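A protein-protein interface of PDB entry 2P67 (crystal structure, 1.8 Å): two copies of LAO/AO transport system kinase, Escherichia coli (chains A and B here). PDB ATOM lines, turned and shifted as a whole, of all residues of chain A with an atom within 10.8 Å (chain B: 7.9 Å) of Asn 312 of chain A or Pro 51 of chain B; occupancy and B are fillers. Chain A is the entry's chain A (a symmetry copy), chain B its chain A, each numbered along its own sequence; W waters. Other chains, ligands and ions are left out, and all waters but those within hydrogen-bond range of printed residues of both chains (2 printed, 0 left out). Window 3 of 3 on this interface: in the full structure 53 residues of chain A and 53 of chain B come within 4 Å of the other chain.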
ATOM      1  N   GLN A 304     -33.261 -38.907 -25.823  1.00  0.00           N
ATOM      2  CA  GLN A 304     -34.044 -37.904 -25.084  1.00  0.00           C
ATOM      3  C   GLN A 304     -33.243 -37.277 -23.937  1.00  0.00           C
ATOM      4  O   GLN A 304     -33.376 -36.088 -23.656  1.00  0.00           O
ATOM      5  CB  GLN A 304     -35.365 -38.500 -24.570  1.00  0.00           C
ATOM      6  CG  GLN A 304     -36.387 -38.832 -25.670  1.00  0.00           C
ATOM      7  CD  GLN A 304     -36.665 -37.675 -26.640  1.00  0.00           C
ATOM      8  OE1 GLN A 304     -36.524 -37.832 -27.848  1.00  0.00           O
ATOM      9  NE2 GLN A 304     -37.057 -36.518 -26.114  1.00  0.00           N
ATOM     10  N   THR A 305     -32.415 -38.088 -23.279  1.00  0.00           N
ATOM     11  CA  THR A 305     -31.541 -37.590 -22.224  1.00  0.00           C
ATOM     12  C   THR A 305     -30.497 -36.640 -22.797  1.00  0.00           C
ATOM     13  O   THR A 305     -30.335 -35.542 -22.286  1.00  0.00           O
ATOM     14  CB  THR A 305     -30.855 -38.729 -21.457  1.00  0.00           C
ATOM     15  OG1 THR A 305     -31.857 -39.568 -20.869  1.00  0.00           O
ATOM     16  CG2 THR A 305     -29.913 -38.168 -20.379  1.00  0.00           C
ATOM     17  N   LEU A 306     -29.814 -37.054 -23.865  1.00  0.00           N
ATOM     18  CA  LEU A 306     -28.875 -36.180 -24.575  1.00  0.00           C
ATOM     19  C   LEU A 306     -29.511 -34.847 -24.957  1.00  0.00           C
ATOM     20  O   LEU A 306     -28.916 -33.791 -24.748  1.00  0.00           O
ATOM     21  CB  LEU A 306     -28.332 -36.853 -25.843  1.00  0.00           C
ATOM     22  CG  LEU A 306     -27.210 -37.892 -25.679  1.00  0.00           C
ATOM     23  CD1 LEU A 306     -26.581 -38.240 -27.035  1.00  0.00           C
ATOM     24  CD2 LEU A 306     -26.164 -37.370 -24.740  1.00  0.00           C
ATOM     25  N   LEU A 307     -30.720 -34.896 -25.498  1.00  0.00           N
ATOM     26  CA  LEU A 307     -31.408 -33.651 -25.899  1.00  0.00           C
ATOM     27  C   LEU A 307     -31.765 -32.756 -24.704  1.00  0.00           C
ATOM     28  O   LEU A 307     -31.637 -31.539 -24.790  1.00  0.00           O
ATOM     29  CB  LEU A 307     -32.649 -33.940 -26.742  1.00  0.00           C
ATOM     30  CG  LEU A 307     -33.270 -32.740 -27.477  1.00  0.00           C
ATOM     31  CD1 LEU A 307     -32.268 -32.033 -28.378  1.00  0.00           C
ATOM     32  CD2 LEU A 307     -34.486 -33.203 -28.295  1.00  0.00           C
ATOM     33  N   ALA A 308     -32.209 -33.369 -23.610  1.00  0.00           N
ATOM     34  CA  ALA A 308     -32.447 -32.651 -22.351  1.00  0.00           C
ATOM     35  C   ALA A 308     -31.205 -31.908 -21.871  1.00  0.00           C
ATOM     36  O   ALA A 308     -31.287 -30.768 -21.456  1.00  0.00           O
ATOM     37  CB  ALA A 308     -32.964 -33.614 -21.264  1.00  0.00           C
ATOM     38  N   VAL A 309     -30.042 -32.554 -21.935  1.00  0.00           N
ATOM     39  CA  VAL A 309     -28.785 -31.897 -21.566  1.00  0.00           C
ATOM     40  C   VAL A 309     -28.441 -30.769 -22.551  1.00  0.00           C
ATOM     41  O   VAL A 309     -28.101 -29.648 -22.146  1.00  0.00           O
ATOM     42  CB  VAL A 309     -27.614 -32.948 -21.424  1.00  0.00           C
ATOM     43  CG1 VAL A 309     -26.286 -32.254 -21.208  1.00  0.00           C
ATOM     44  CG2 VAL A 309     -27.915 -33.953 -20.284  1.00  0.00           C
ATOM     45  N   LYS A 310     -28.595 -31.036 -23.844  1.00  0.00           N
ATOM     46  CA  LYS A 310     -28.272 -30.037 -24.853  1.00  0.00           C
ATOM     47  C   LYS A 310     -29.134 -28.791 -24.669  1.00  0.00           C
ATOM     48  O   LYS A 310     -28.648 -27.666 -24.853  1.00  0.00           O
ATOM     49  CB  LYS A 310     -28.499 -30.640 -26.239  1.00  0.00           C
ATOM     50  CG  LYS A 310     -28.078 -29.808 -27.410  1.00  0.00           C
ATOM     51  CD  LYS A 310     -28.247 -30.654 -28.684  1.00  0.00           C
ATOM     52  CE  LYS A 310     -28.140 -29.775 -29.916  1.00  0.00           C
ATOM     53  NZ  LYS A 310     -27.188 -30.269 -30.937  1.00  0.00           N
ATOM     54  N   ASN A 311     -30.401 -28.995 -24.294  1.00  0.00           N
ATOM     55  CA  ASN A 311     -31.369 -27.902 -24.121  1.00  0.00           C
ATOM     56  C   ASN A 311     -31.371 -27.277 -22.708  1.00  0.00           C
ATOM     57  O   ASN A 311     -32.250 -26.462 -22.377  1.00  0.00           O
ATOM     58  CB  ASN A 311     -32.783 -28.400 -24.477  1.00  0.00           C
ATOM     59  CG  ASN A 311     -33.082 -28.333 -25.961  1.00  0.00           C
ATOM     60  OD1 ASN A 311     -32.558 -27.486 -26.690  1.00  0.00           O
ATOM     61  ND2 ASN A 311     -33.949 -29.229 -26.415  1.00  0.00           N
ATOM     62  N   ASN A 312     -30.381 -27.642 -21.891  1.00  0.00           N
ATOM     63  CA  ASN A 312     -30.160 -27.011 -20.573  1.00  0.00           C
ATOM     64  C   ASN A 312     -31.254 -27.272 -19.537  1.00  0.00           C
ATOM     65  O   ASN A 312     -31.408 -26.497 -18.573  1.00  0.00           O
ATOM     66  CB  ASN A 312     -29.927 -25.499 -20.709  1.00  0.00           C
ATOM     67  CG  ASN A 312     -28.843 -25.169 -21.700  1.00  0.00           C
ATOM     68  OD1 ASN A 312     -27.798 -25.813 -21.716  1.00  0.00           O
ATOM     69  ND2 ASN A 312     -29.085 -24.162 -22.540  1.00  0.00           N
ATOM     70  N   THR A 313     -31.989 -28.363 -19.725  1.00  0.00           N
ATOM     71  CA  THR A 313     -33.031 -28.741 -18.767  1.00  0.00           C
ATOM     72  C   THR A 313     -32.535 -29.681 -17.663  1.00  0.00           C
ATOM     73  O   THR A 313     -33.166 -29.786 -16.615  1.00  0.00           O
ATOM     74  CB  THR A 313     -34.289 -29.330 -19.456  1.00  0.00           C
ATOM     75  OG1 THR A 313     -33.981 -30.619 -20.000  1.00  0.00           O
ATOM     76  CG2 THR A 313     -34.784 -28.395 -20.552  1.00  0.00           C
ATOM     77  N   LEU A 314     -31.420 -30.363 -17.912  1.00  0.00           N
ATOM     78  CA  LEU A 314     -30.812 -31.295 -16.957  1.00  0.00           C
ATOM     79  C   LEU A 314     -29.323 -31.053 -16.953  1.00  0.00           C
ATOM     80  O   LEU A 314     -28.727 -30.817 -18.018  1.00  0.00           O
ATOM     81  CB  LEU A 314     -30.982 -32.750 -17.416  1.00  0.00           C
ATOM     82  CG  LEU A 314     -32.302 -33.507 -17.483  1.00  0.00           C
ATOM     83  CD1 LEU A 314     -32.012 -34.943 -17.911  1.00  0.00           C
ATOM     84  CD2 LEU A 314     -32.982 -33.496 -16.129  1.00  0.00           C
ATOM     85  N   SER A 315     -28.702 -31.184 -15.780  1.00  0.00           N
ATOM     86  CA  SER A 315     -27.249 -31.210 -15.721  1.00  0.00           C
ATOM     87  C   SER A 315     -26.739 -32.559 -16.238  1.00  0.00           C
ATOM     88  O   SER A 315     -27.466 -33.542 -16.225  1.00  0.00           O
ATOM     89  CB  SER A 315     -26.743 -31.018 -14.279  1.00  0.00           C
ATOM     90  OG  SER A 315     -27.201 -32.086 -13.478  1.00  0.00           O
ATOM     91  N   PRO A 316     -25.475 -32.605 -16.686  1.00  0.00           N
ATOM     92  CA  PRO A 316     -24.830 -33.884 -16.990  1.00  0.00           C
ATOM     93  C   PRO A 316     -24.947 -34.916 -15.848  1.00  0.00           C
ATOM     94  O   PRO A 316     -25.265 -36.078 -16.114  1.00  0.00           O
ATOM     95  CB  PRO A 316     -23.385 -33.476 -17.260  1.00  0.00           C
ATOM     96  CG  PRO A 316     -23.526 -32.079 -17.841  1.00  0.00           C
ATOM     97  CD  PRO A 316     -24.598 -31.458 -16.995  1.00  0.00           C
ATOM     98  N   THR A 318     -27.333 -35.309 -13.607  1.00  0.00           N
ATOM     99  CA  THR A 318     -28.684 -35.858 -13.615  1.00  0.00           C
ATOM    100  C   THR A 318     -28.894 -36.723 -14.838  1.00  0.00           C
ATOM    101  O   THR A 318     -29.480 -37.801 -14.739  1.00  0.00           O
ATOM    102  CB  THR A 318     -29.767 -34.753 -13.511  1.00  0.00           C
ATOM    103  OG1 THR A 318     -29.673 -34.166 -12.222  1.00  0.00           O
ATOM    104  CG2 THR A 318     -31.171 -35.334 -13.646  1.00  0.00           C
ATOM    105  N   GLY A 319     -28.387 -36.268 -15.985  1.00  0.00           N
ATOM    106  CA  GLY A 319     -28.437 -37.081 -17.197  1.00  0.00           C
ATOM    107  C   GLY A 319     -27.860 -38.473 -16.947  1.00  0.00           C
ATOM    108  O   GLY A 319     -28.485 -39.498 -17.279  1.00  0.00           O
ATOM    109  N   ARG B  17     -25.386 -15.829  -9.267  1.00  0.00           N
ATOM    110  CA  ARG B  17     -25.324 -15.181 -10.580  1.00  0.00           C
ATOM    111  C   ARG B  17     -24.853 -13.734 -10.516  1.00  0.00           C
ATOM    112  O   ARG B  17     -24.320 -13.200 -11.498  1.00  0.00           O
ATOM    113  CB  ARG B  17     -26.692 -15.240 -11.259  1.00  0.00           C
ATOM    114  CG  ARG B  17     -27.159 -16.622 -11.607  1.00  0.00           C
ATOM    115  CD  ARG B  17     -28.583 -16.549 -12.139  1.00  0.00           C
ATOM    116  NE  ARG B  17     -28.637 -15.766 -13.379  1.00  0.00           N
ATOM    117  CZ  ARG B  17     -29.727 -15.151 -13.844  1.00  0.00           C
ATOM    118  NH1 ARG B  17     -30.871 -15.213 -13.172  1.00  0.00           N
ATOM    119  NH2 ARG B  17     -29.672 -14.475 -14.989  1.00  0.00           N
ATOM    120  N   LEU B  45     -29.523 -27.827  -7.627  1.00  0.00           N
ATOM    121  CA  LEU B  45     -28.766 -26.614  -7.955  1.00  0.00           C
ATOM    122  C   LEU B  45     -28.169 -26.716  -9.363  1.00  0.00           C
ATOM    123  O   LEU B  45     -28.267 -25.782 -10.167  1.00  0.00           O
ATOM    124  CB  LEU B  45     -27.626 -26.408  -6.933  1.00  0.00           C
ATOM    125  CG  LEU B  45     -26.552 -25.360  -7.241  1.00  0.00           C
ATOM    126  CD1 LEU B  45     -27.202 -24.004  -7.433  1.00  0.00           C
ATOM    127  CD2 LEU B  45     -25.494 -25.300  -6.127  1.00  0.00           C
ATOM    128  N   LEU B  46     -27.523 -27.845  -9.641  1.00  0.00           N
ATOM    129  CA  LEU B  46     -26.837 -28.017 -10.926  1.00  0.00           C
ATOM    130  C   LEU B  46     -27.846 -28.018 -12.080  1.00  0.00           C
ATOM    131  O   LEU B  46     -27.624 -27.348 -13.091  1.00  0.00           O
ATOM    132  CB  LEU B  46     -25.958 -29.264 -10.927  1.00  0.00           C
ATOM    133  CG  LEU B  46     -24.688 -29.159 -10.057  1.00  0.00           C
ATOM    134  CD1 LEU B  46     -24.130 -30.548  -9.740  1.00  0.00           C
ATOM    135  CD2 LEU B  46     -23.622 -28.218 -10.662  1.00  0.00           C
ATOM    136  N   ASP B  47     -28.962 -28.728 -11.917  1.00  0.00           N
ATOM    137  CA  ASP B  47     -30.057 -28.657 -12.913  1.00  0.00           C
ATOM    138  C   ASP B  47     -30.500 -27.217 -13.124  1.00  0.00           C
ATOM    139  O   ASP B  47     -30.627 -26.736 -14.260  1.00  0.00           O
ATOM    140  CB  ASP B  47     -31.273 -29.497 -12.478  1.00  0.00           C
ATOM    141  CG  ASP B  47     -31.023 -30.982 -12.556  1.00  0.00           C
ATOM    142  OD1 ASP B  47     -30.069 -31.409 -13.232  1.00  0.00           O
ATOM    143  OD2 ASP B  47     -31.771 -31.744 -11.913  1.00  0.00           O
ATOM    144  N   ALA B  48     -30.719 -26.508 -12.020  1.00  0.00           N
ATOM    145  CA  ALA B  48     -31.253 -25.156 -12.102  1.00  0.00           C
ATOM    146  C   ALA B  48     -30.329 -24.153 -12.807  1.00  0.00           C
ATOM    147  O   ALA B  48     -30.816 -23.234 -13.473  1.00  0.00           O
ATOM    148  CB  ALA B  48     -31.668 -24.646 -10.725  1.00  0.00           C
ATOM    149  N   ILE B  49     -29.008 -24.327 -12.692  1.00  0.00           N
ATOM    150  CA  ILE B  49     -28.103 -23.327 -13.243  1.00  0.00           C
ATOM    151  C   ILE B  49     -27.743 -23.519 -14.718  1.00  0.00           C
ATOM    152  O   ILE B  49     -27.125 -22.635 -15.313  1.00  0.00           O
ATOM    153  CB  ILE B  49     -26.780 -23.130 -12.408  1.00  0.00           C
ATOM    154  CG1 ILE B  49     -25.938 -24.424 -12.394  1.00  0.00           C
ATOM    155  CG2 ILE B  49     -27.086 -22.580 -11.010  1.00  0.00           C
ATOM    156  CD1 ILE B  49     -24.473 -24.215 -12.072  1.00  0.00           C
ATOM    157  N   MET B  50     -28.126 -24.661 -15.299  1.00  0.00           N
ATOM    158  CA  MET B  50     -27.712 -24.987 -16.663  1.00  0.00           C
ATOM    159  C   MET B  50     -27.991 -23.843 -17.670  1.00  0.00           C
ATOM    160  O   MET B  50     -27.135 -23.516 -18.483  1.00  0.00           O
ATOM    161  CB  MET B  50     -28.267 -26.352 -17.130  1.00  0.00           C
ATOM    162  CG  MET B  50     -27.869 -27.553 -16.251  1.00  0.00           C
ATOM    163  SD  MET B  50     -26.040 -27.615 -15.938  1.00  0.00           S
ATOM    164  CE  MET B  50     -25.533 -27.735 -17.583  1.00  0.00           C
ATOM    165  N   PRO B  51     -29.176 -23.203 -17.605  1.00  0.00           N
ATOM    166  CA  PRO B  51     -29.424 -22.102 -18.565  1.00  0.00           C
ATOM    167  C   PRO B  51     -28.481 -20.889 -18.460  1.00  0.00           C
ATOM    168  O   PRO B  51     -28.387 -20.120 -19.419  1.00  0.00           O
ATOM    169  CB  PRO B  51     -30.875 -21.690 -18.256  1.00  0.00           C
ATOM    170  CG  PRO B  51     -31.479 -22.897 -17.638  1.00  0.00           C
ATOM    171  CD  PRO B  51     -30.362 -23.460 -16.769  1.00  0.00           C
ATOM    172  N   TYR B  52     -27.790 -20.738 -17.327  1.00  0.00           N
ATOM    173  CA  TYR B  52     -26.894 -19.597 -17.074  1.00  0.00           C
ATOM    174  C   TYR B  52     -25.437 -19.903 -17.447  1.00  0.00           C
ATOM    175  O   TYR B  52     -24.556 -19.029 -17.388  1.00  0.00           O
ATOM    176  CB  TYR B  52     -27.007 -19.162 -15.601  1.00  0.00           C
ATOM    177  CG  TYR B  52     -28.443 -19.073 -15.119  1.00  0.00           C
ATOM    178  CD1 TYR B  52     -29.299 -18.061 -15.571  1.00  0.00           C
ATOM    179  CD2 TYR B  52     -28.960 -20.020 -14.242  1.00  0.00           C
ATOM    180  CE1 TYR B  52     -30.643 -17.995 -15.129  1.00  0.00           C
ATOM    181  CE2 TYR B  52     -30.289 -19.964 -13.808  1.00  0.00           C
ATOM    182  CZ  TYR B  52     -31.117 -18.955 -14.257  1.00  0.00           C
ATOM    183  OH  TYR B  52     -32.425 -18.908 -13.811  1.00  0.00           O
ATOM    184  N   CYS B  53     -25.178 -21.138 -17.858  1.00  0.00           N
ATOM    185  CA  CYS B  53     -23.818 -21.524 -18.254  1.00  0.00           C
ATOM    186  C   CYS B  53     -23.528 -21.287 -19.756  1.00  0.00           C
ATOM    187  O   CYS B  53     -24.444 -20.950 -20.530  1.00  0.00           O
ATOM    188  CB  CYS B  53     -23.571 -22.971 -17.819  1.00  0.00           C
ATOM    189  SG  CYS B  53     -23.751 -23.151 -16.030  1.00  0.00           S
ATOM    190  N   GLY B  54     -22.268 -21.441 -20.181  1.00  0.00           N
ATOM    191  CA  GLY B  54     -21.949 -21.487 -21.614  1.00  0.00           C
ATOM    192  C   GLY B  54     -21.449 -20.223 -22.311  1.00  0.00           C
ATOM    193  O   GLY B  54     -21.259 -20.210 -23.541  1.00  0.00           O
ATOM    194  N   ASN B  55     -21.232 -19.164 -21.545  1.00  0.00           N
ATOM    195  CA  ASN B  55     -20.706 -17.908 -22.077  1.00  0.00           C
ATOM    196  C   ASN B  55     -19.403 -17.514 -21.392  1.00  0.00           C
ATOM    197  O   ASN B  55     -19.168 -16.344 -21.051  1.00  0.00           O
ATOM    198  CB  ASN B  55     -21.755 -16.799 -21.958  1.00  0.00           C
ATOM    199  CG  ASN B  55     -22.669 -16.737 -23.186  1.00  0.00           C
ATOM    200  OD1 ASN B  55     -22.235 -16.388 -24.297  1.00  0.00           O
ATOM    201  ND2 ASN B  55     -23.923 -17.096 -22.995  1.00  0.00           N
ATOM    202  N   ALA B 146     -21.980 -19.965 -14.214  1.00  0.00           N
ATOM    203  CA  ALA B 146     -23.227 -19.379 -13.714  1.00  0.00           C
ATOM    204  C   ALA B 146     -22.947 -18.115 -12.886  1.00  0.00           C
ATOM    205  O   ALA B 146     -23.737 -17.157 -12.921  1.00  0.00           O
ATOM    206  CB  ALA B 146     -24.026 -20.421 -12.925  1.00  0.00           C
HETATM  207  O   HOH W   1     -32.651 -26.189 -16.180  1.00  0.00           O
HETATM  208  O   HOH W   2     -25.328 -24.890 -21.022  1.00  0.00           O
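OG of Ser 315 of chain A lies within hydrogen-bond range of N of Thr 318 of chain A, 3.2 Å away.
Water W1 bridges the backbone carbonyl oxygen (O) of Asn 312 of chain A and the backbone carbonyl oxygen (O) of Asp 47 of chain B. Water W2 bridges the side-chain amide oxygen (OD1) of Asn 312 of chain A (2.7 Å) and the backbone carbonyl oxygen (O) of Met 50 of chain B (3.4 Å).
Asn 312 of chain A touches Met 50 of chain B. Pro 51 of chain B touches Asn 312 of chain A (CD to O, 3.7 Å). Asp 47 of chain B touches Leu 314 of chain A (OD1 to CA, 3.8 Å). Met 50 of chain B touches Leu 314 of chain A. CB of Ser 315 of chain A touches CB of Leu 46 of chain B, at 3.9 Å. CA of Ser 315 of chain A touches CG of Met 50 of chain B, at 3.7 Å. Met 50 of chain B touches Pro 316 of chain A (CE to CD, 3.9 Å).
Hydrophobic or aromatic side chains of chain B that line the printed part of chain A: Leu 46, Met 50 and Pro 51. Along chain B the printed residues that touch a printed residue of chain A span positions 46 to 51. Of the 15 printed residues of chain A, 5 touch a printed residue of chain B. Printed residues of chain A that touch a printed residue of chain B: Asn 312, Leu 314, Ser 315, Pro 316 and Thr 318. Hydrophobic or aromatic side chains of chain A within 4 Å of the printed part of chain B: Pro 316. Among the printed residues, 9 pairs touch across the chains. Among the printed residues, no Asp or Glu carboxylate lies within 4 Å of a Lys or Arg side-chain nitrogen of the other chain.
Lys 310 of chain A touches none of the printed residues of chain B. Of chain B, only Met 50 and Pro 51 come within 4 Å of Asn 312 of chain A. Printed residues of chain B within 4 Å of Leu 314 of chain A: Asp 47 (3.8 Å) and Met 50 (3.8 Å). Printed residues of chain B within 4 Å of Thr 318 of chain A: Asp 47 (3.0 Å). Printed residues of chain A within 4 Å of Leu 46 of chain B: Ser 315 (3.9 Å). Printed residues of chain A within 4 Å of Asp 47 of chain B: Leu 314, Ser 315 and Thr 318. No residue of chain A comes within 4 Å of Ala 48 of chain B. Pro 51 of chain B touches just one residue of chain A: Asn 312. No residue of chain A comes within 4 Å of Cys 53 of chain B. The nearest residue of chain B that does not touch Asn 312 of chain A is Asp 47 of chain B (4.4 Å).
No position is printed for both chains. Of the 9 pairs that touch across the chains among the printed residues, none has its exchanged pair printed and touching as well.
The side-chain carboxylate (OD1) of Asp 47 of chain B sits at hydrogen-bond distance from the backbone NH (N) of Ser 315 of chain A, 2.9 Å away. OD1 of Asp 47 of chain B lies within hydrogen-bond range of OG1 of Thr 318 of chain A (3.0 Å).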
